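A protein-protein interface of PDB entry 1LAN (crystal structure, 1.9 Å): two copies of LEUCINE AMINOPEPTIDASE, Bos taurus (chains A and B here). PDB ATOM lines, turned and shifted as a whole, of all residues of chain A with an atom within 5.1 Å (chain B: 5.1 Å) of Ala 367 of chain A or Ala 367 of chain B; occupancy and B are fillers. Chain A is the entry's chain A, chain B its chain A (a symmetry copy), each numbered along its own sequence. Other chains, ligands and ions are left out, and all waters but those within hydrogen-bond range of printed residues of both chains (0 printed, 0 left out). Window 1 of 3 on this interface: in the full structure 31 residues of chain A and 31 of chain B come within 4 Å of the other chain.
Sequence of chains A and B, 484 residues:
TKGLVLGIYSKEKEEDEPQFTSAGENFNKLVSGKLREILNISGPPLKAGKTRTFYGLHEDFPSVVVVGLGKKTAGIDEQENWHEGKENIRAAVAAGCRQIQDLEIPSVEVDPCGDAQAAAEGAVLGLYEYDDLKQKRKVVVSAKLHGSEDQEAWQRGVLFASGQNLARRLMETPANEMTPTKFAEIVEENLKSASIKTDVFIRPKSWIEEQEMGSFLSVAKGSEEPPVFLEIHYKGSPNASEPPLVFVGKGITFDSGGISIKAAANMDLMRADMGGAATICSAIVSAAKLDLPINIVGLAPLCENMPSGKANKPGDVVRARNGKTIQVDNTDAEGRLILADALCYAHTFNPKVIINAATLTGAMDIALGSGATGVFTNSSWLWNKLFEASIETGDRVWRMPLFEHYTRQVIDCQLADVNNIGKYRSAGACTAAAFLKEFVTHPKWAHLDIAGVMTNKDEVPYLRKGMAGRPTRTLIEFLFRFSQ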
ATOM      1  N   ALA A 363     -22.761  -9.187 -30.424  1.00  0.00           N
ATOM      2  CA  ALA A 363     -21.759  -9.384 -29.370  1.00  0.00           C
ATOM      3  C   ALA A 363     -21.857 -10.762 -28.701  1.00  0.00           C
ATOM      4  O   ALA A 363     -20.849 -11.322 -28.291  1.00  0.00           O
ATOM      5  CB  ALA A 363     -21.856  -8.268 -28.310  1.00  0.00           C
ATOM      6  N   MET A 364     -23.064 -11.307 -28.580  1.00  0.00           N
ATOM      7  CA  MET A 364     -23.232 -12.623 -27.968  1.00  0.00           C
ATOM      8  C   MET A 364     -22.583 -13.671 -28.868  1.00  0.00           C
ATOM      9  O   MET A 364     -21.931 -14.592 -28.378  1.00  0.00           O
ATOM     10  CB  MET A 364     -24.720 -12.979 -27.769  1.00  0.00           C
ATOM     11  CG  MET A 364     -24.961 -14.279 -26.957  1.00  0.00           C
ATOM     12  SD  MET A 364     -24.500 -14.060 -25.187  1.00  0.00           S
ATOM     13  CE  MET A 364     -23.339 -15.254 -25.023  1.00  0.00           C
ATOM     14  N   ASP A 365     -22.738 -13.527 -30.182  1.00  0.00           N
ATOM     15  CA  ASP A 365     -22.128 -14.487 -31.103  1.00  0.00           C
ATOM     16  C   ASP A 365     -20.600 -14.393 -30.987  1.00  0.00           C
ATOM     17  O   ASP A 365     -19.901 -15.407 -30.925  1.00  0.00           O
ATOM     18  CB  ASP A 365     -22.590 -14.245 -32.544  1.00  0.00           C
ATOM     19  CG  ASP A 365     -21.997 -15.253 -33.512  1.00  0.00           C
ATOM     20  OD1 ASP A 365     -22.205 -16.467 -33.313  1.00  0.00           O
ATOM     21  OD2 ASP A 365     -21.270 -14.852 -34.437  1.00  0.00           O
ATOM     22  N   ILE A 366     -20.088 -13.175 -30.910  1.00  0.00           N
ATOM     23  CA  ILE A 366     -18.653 -12.971 -30.739  1.00  0.00           C
ATOM     24  C   ILE A 366     -18.210 -13.571 -29.394  1.00  0.00           C
ATOM     25  O   ILE A 366     -17.138 -14.150 -29.307  1.00  0.00           O
ATOM     26  CB  ILE A 366     -18.294 -11.460 -30.791  1.00  0.00           C
ATOM     27  CG1 ILE A 366     -18.625 -10.871 -32.165  1.00  0.00           C
ATOM     28  CG2 ILE A 366     -16.832 -11.234 -30.459  1.00  0.00           C
ATOM     29  CD1 ILE A 366     -17.998 -11.631 -33.328  1.00  0.00           C
ATOM     30  N   ALA A 367     -19.067 -13.492 -28.375  1.00  0.00           N
ATOM     31  CA  ALA A 367     -18.753 -14.014 -27.042  1.00  0.00           C
ATOM     32  C   ALA A 367     -18.654 -15.545 -26.924  1.00  0.00           C
ATOM     33  O   ALA A 367     -17.621 -16.066 -26.501  1.00  0.00           O
ATOM     34  CB  ALA A 367     -19.761 -13.473 -26.012  1.00  0.00           C
ATOM     35  N   LEU A 368     -19.712 -16.261 -27.305  1.00  0.00           N
ATOM     36  CA  LEU A 368     -19.741 -17.723 -27.185  1.00  0.00           C
ATOM     37  C   LEU A 368     -20.049 -18.514 -28.464  1.00  0.00           C
ATOM     38  O   LEU A 368     -20.025 -19.753 -28.442  1.00  0.00           O
ATOM     39  CB  LEU A 368     -20.765 -18.141 -26.117  1.00  0.00           C
ATOM     40  CG  LEU A 368     -20.646 -17.596 -24.688  1.00  0.00           C
ATOM     41  CD1 LEU A 368     -21.792 -18.113 -23.827  1.00  0.00           C
ATOM     42  CD2 LEU A 368     -19.336 -18.030 -24.099  1.00  0.00           C
ATOM     43  N   GLY A 369     -20.359 -17.823 -29.561  1.00  0.00           N
ATOM     44  CA  GLY A 369     -20.681 -18.522 -30.799  1.00  0.00           C
ATOM     45  C   GLY A 369     -21.882 -19.457 -30.637  1.00  0.00           C
ATOM     46  O   GLY A 369     -22.851 -19.124 -29.945  1.00  0.00           O
ATOM     47  N   MET A 400     -24.196 -15.422 -18.021  1.00  0.00           N
ATOM     48  CA  MET A 400     -23.505 -14.156 -18.312  1.00  0.00           C
ATOM     49  C   MET A 400     -23.899 -13.177 -17.187  1.00  0.00           C
ATOM     50  O   MET A 400     -25.014 -13.240 -16.659  1.00  0.00           O
ATOM     51  CB  MET A 400     -23.905 -13.633 -19.693  1.00  0.00           C
ATOM     52  CG  MET A 400     -23.452 -14.527 -20.856  1.00  0.00           C
ATOM     53  SD  MET A 400     -21.653 -14.529 -21.130  1.00  0.00           S
ATOM     54  CE  MET A 400     -21.488 -12.996 -22.086  1.00  0.00           C
ATOM     55  N   ALA A 427     -18.652  -5.165 -24.234  1.00  0.00           N
ATOM     56  CA  ALA A 427     -19.720  -5.930 -23.572  1.00  0.00           C
ATOM     57  C   ALA A 427     -21.146  -5.699 -24.070  1.00  0.00           C
ATOM     58  O   ALA A 427     -22.091  -5.594 -23.273  1.00  0.00           O
ATOM     59  CB  ALA A 427     -19.659  -5.711 -22.047  1.00  0.00           C
ATOM     60  N   CYS A 430     -23.948  -7.706 -22.517  1.00  0.00           N
ATOM     61  CA  CYS A 430     -24.187  -7.342 -21.108  1.00  0.00           C
ATOM     62  C   CYS A 430     -24.953  -6.010 -20.914  1.00  0.00           C
ATOM     63  O   CYS A 430     -25.808  -5.891 -20.024  1.00  0.00           O
ATOM     64  CB  CYS A 430     -22.872  -7.325 -20.324  1.00  0.00           C
ATOM     65  SG  CYS A 430     -21.955  -8.870 -20.373  1.00  0.00           S
ATOM     66  N   ALA B 363     -12.195 -10.134 -28.774  1.00  0.00           N
ATOM     67  CA  ALA B 363     -13.479 -10.799 -28.519  1.00  0.00           C
ATOM     68  C   ALA B 363     -13.845 -10.842 -27.030  1.00  0.00           C
ATOM     69  O   ALA B 363     -15.017 -10.782 -26.680  1.00  0.00           O
ATOM     70  CB  ALA B 363     -13.482 -12.224 -29.111  1.00  0.00           C
ATOM     71  N   MET B 364     -12.853 -10.954 -26.151  1.00  0.00           N
ATOM     72  CA  MET B 364     -13.126 -10.986 -24.716  1.00  0.00           C
ATOM     73  C   MET B 364     -13.673  -9.626 -24.289  1.00  0.00           C
ATOM     74  O   MET B 364     -14.603  -9.556 -23.487  1.00  0.00           O
ATOM     75  CB  MET B 364     -11.857 -11.300 -23.897  1.00  0.00           C
ATOM     76  CG  MET B 364     -12.116 -11.530 -22.384  1.00  0.00           C
ATOM     77  SD  MET B 364     -13.022 -13.107 -22.090  1.00  0.00           S
ATOM     78  CE  MET B 364     -14.386 -12.535 -21.308  1.00  0.00           C
ATOM     79  N   ASP B 365     -13.118  -8.546 -24.834  1.00  0.00           N
ATOM     80  CA  ASP B 365     -13.606  -7.212 -24.483  1.00  0.00           C
ATOM     81  C   ASP B 365     -15.054  -7.062 -24.969  1.00  0.00           C
ATOM     82  O   ASP B 365     -15.921  -6.563 -24.249  1.00  0.00           O
ATOM     83  CB  ASP B 365     -12.707  -6.119 -25.071  1.00  0.00           C
ATOM     84  CG  ASP B 365     -13.174  -4.727 -24.687  1.00  0.00           C
ATOM     85  OD1 ASP B 365     -13.269  -4.440 -23.476  1.00  0.00           O
ATOM     86  OD2 ASP B 365     -13.510  -3.931 -25.581  1.00  0.00           O
ATOM     87  N   ILE B 366     -15.323  -7.538 -26.175  1.00  0.00           N
ATOM     88  CA  ILE B 366     -16.679  -7.500 -26.713  1.00  0.00           C
ATOM     89  C   ILE B 366     -17.600  -8.363 -25.835  1.00  0.00           C
ATOM     90  O   ILE B 366     -18.741  -7.995 -25.602  1.00  0.00           O
ATOM     91  CB  ILE B 366     -16.711  -8.011 -28.181  1.00  0.00           C
ATOM     92  CG1 ILE B 366     -15.888  -7.096 -29.092  1.00  0.00           C
ATOM     93  CG2 ILE B 366     -18.134  -8.120 -28.690  1.00  0.00           C
ATOM     94  CD1 ILE B 366     -16.283  -5.626 -29.008  1.00  0.00           C
ATOM     95  N   ALA B 367     -17.078  -9.466 -25.298  1.00  0.00           N
ATOM     96  CA  ALA B 367     -17.860 -10.375 -24.456  1.00  0.00           C
ATOM     97  C   ALA B 367     -18.280  -9.826 -23.081  1.00  0.00           C
ATOM     98  O   ALA B 367     -19.471  -9.789 -22.769  1.00  0.00           O
ATOM     99  CB  ALA B 367     -17.112 -11.709 -24.281  1.00  0.00           C
ATOM    100  N   LEU B 368     -17.315  -9.393 -22.270  1.00  0.00           N
ATOM    101  CA  LEU B 368     -17.602  -8.899 -20.919  1.00  0.00           C
ATOM    102  C   LEU B 368     -17.093  -7.493 -20.576  1.00  0.00           C
ATOM    103  O   LEU B 368     -17.359  -6.994 -19.473  1.00  0.00           O
ATOM    104  CB  LEU B 368     -17.033  -9.872 -19.874  1.00  0.00           C
ATOM    105  CG  LEU B 368     -17.456 -11.348 -19.889  1.00  0.00           C
ATOM    106  CD1 LEU B 368     -16.731 -12.119 -18.793  1.00  0.00           C
ATOM    107  CD2 LEU B 368     -18.938 -11.441 -19.677  1.00  0.00           C
ATOM    108  N   GLY B 369     -16.351  -6.862 -21.486  1.00  0.00           N
ATOM    109  CA  GLY B 369     -15.823  -5.533 -21.207  1.00  0.00           C
ATOM    110  C   GLY B 369     -14.923  -5.520 -19.969  1.00  0.00           C
ATOM    111  O   GLY B 369     -14.153  -6.459 -19.739  1.00  0.00           O
ATOM    112  N   MET B 400     -15.652 -18.859 -18.444  1.00  0.00           N
ATOM    113  CA  MET B 400     -15.972 -18.993 -19.874  1.00  0.00           C
ATOM    114  C   MET B 400     -15.743 -20.475 -20.235  1.00  0.00           C
ATOM    115  O   MET B 400     -14.863 -21.132 -19.668  1.00  0.00           O
ATOM    116  CB  MET B 400     -15.096 -18.058 -20.709  1.00  0.00           C
ATOM    117  CG  MET B 400     -15.353 -16.566 -20.455  1.00  0.00           C
ATOM    118  SD  MET B 400     -16.960 -15.977 -21.073  1.00  0.00           S
ATOM    119  CE  MET B 400     -16.543 -15.730 -22.821  1.00  0.00           C
ATOM    120  N   ALA B 427     -17.078 -16.523 -31.370  1.00  0.00           N
ATOM    121  CA  ALA B 427     -16.416 -16.999 -30.145  1.00  0.00           C
ATOM    122  C   ALA B 427     -14.890 -16.924 -30.111  1.00  0.00           C
ATOM    123  O   ALA B 427     -14.216 -17.858 -29.649  1.00  0.00           O
ATOM    124  CB  ALA B 427     -16.874 -18.435 -29.821  1.00  0.00           C
ATOM    125  N   CYS B 430     -13.099 -18.011 -26.963  1.00  0.00           N
ATOM    126  CA  CYS B 430     -13.215 -19.461 -26.722  1.00  0.00           C
ATOM    127  C   CYS B 430     -12.298 -20.332 -27.616  1.00  0.00           C
ATOM    128  O   CYS B 430     -11.733 -21.337 -27.160  1.00  0.00           O
ATOM    129  CB  CYS B 430     -14.673 -19.913 -26.844  1.00  0.00           C
ATOM    130  SG  CYS B 430     -15.815 -19.054 -25.753  1.00  0.00           S
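Among the printed residues, merely in contact across the chains: Ala 427 of chain A with Leu 368 of chain B (3.5 Å), Leu 368 of chain A with Ala 427 of chain B (3.5 Å), Ala 427 of chain A with Gly 369 of chain B (3.5 Å), Gly 369 of chain A with Ala 427 of chain B (3.5 Å), Ala 367 of chain A with Ala 367 of chain B (3.6 Å), Ala 363 of chain A with Ile 366 of chain B (3.7 Å), Ile 366 of chain A with Ala 363 of chain B (3.7 Å), Ile 366 of chain A with Ile 366 of chain B (3.8 Å), Met 400 of chain A with Leu 368 of chain B (3.8 Å), Leu 368 of chain A with Met 400 of chain B (3.8 Å), Ala 367 of chain A with Met 400 of chain B (3.8 Å), Met 400 of chain A with Ala 367 of chain B (3.8 Å), Ala 427 of chain A with Ala 367 of chain B (3.9 Å) and Ala 367 of chain A with Ala 427 of chain B (3.9 Å).
O of Asp 365 of chain A sits at hydrogen-bond distance from N of Ala 427 of chain B, at 3.1 Å.
The backbone carbonyl oxygen of Ile 366 of chain A lies close to the backbone NH of Ala 427 of chain B, 3.1 Å away.
The backbone carbonyl oxygen (O) of Ala 367 of chain A is in hydrogen-bond range of the side-chain sulfur (SG) of Cys 430 of chain B.
N of Ala 427 of chain A lies within hydrogen-bond range of O of Asp 365 of chain B (3.1 Å).
The backbone carbonyl oxygen of Ile 366 of chain B sits close to the backbone NH of Ala 427 of chain A.
The side-chain sulfur of Cys 430 of chain A lies within hydrogen-bond range of the backbone carbonyl oxygen of Ala 367 of chain B.
Of chain B, only Ala 367, Met 400, Ala 427 and Cys 430 come within 4 Å of Ala 367 of chain A.
Of chain A, only Ala 367, Met 400, Ala 427 and Cys 430 come within 4 Å of Ala 367 of chain B.
Of the printed residues of chain B, Met 400 of chain A touches Ala 367 (3.8 Å) and Leu 368 (3.8 Å).
Of the printed residues of chain A, Ile 366 of chain B touches Ala 363 (3.7 Å), Ile 366 (3.8 Å) and Ala 427 (3.1 Å).
Of the printed residues of chain B, Cys 430 of chain A touches Ala 367.
Of the printed residues of chain A, Ala 427 of chain B touches Asp 365 (3.1 Å), Ile 366 (3.1 Å), Ala 367 (3.9 Å), Leu 368 (3.5 Å) and Gly 369 (3.5 Å).
Printed residues of chain A within 4 Å of Cys 430 of chain B: Ala 367 (3.6 Å).
The nearest printed residue of chain B that does not touch Gly 369 of chain A is Cys 430 of chain B (6.1 Å).
Ile 366 of chain B touches its own counterpart, Ile 366 of chain A.
Ala 367 of chain A touches Cys 430 of chain B, and with the chains exchanged Cys 430 of chain A touches Ala 367 of chain B.
Leu 368 of chain A touches Met 400 of chain B, and with the chains exchanged Met 400 of chain A touches Leu 368 of chain B.
Gly 369 of chain A touches Ala 427 of chain B, and with the chains exchanged Ala 427 of chain A touches Gly 369 of chain B.
Of the 20 pairs that touch across the chains among the printed residues, 20 have their exchanged pair printed and touching as well.
Hydrophobic or aromatic side chains of chain A within 4 Å of the printed part of chain B: Ala 363, Ile 366, Ala 367, Leu 368, Met 400 and Ala 427.
Along chain A the printed residues that touch a printed residue of chain B span positions 363 to 430.
Printed residues of chain B that touch a printed residue of chain A: Ala 363, Asp 365, Ile 366, Ala 367, Leu 368, Gly 369, Met 400, Ala 427 and Cys 430.
Along chain B the printed residues that touch a printed residue of chain A span positions 363 to 430.
Among the printed residues, 20 pairs touch across the chains.
Among the printed residues, no Asp or Glu carboxylate lies within 4 Å of a Lys or Arg side-chain nitrogen of the other chain.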
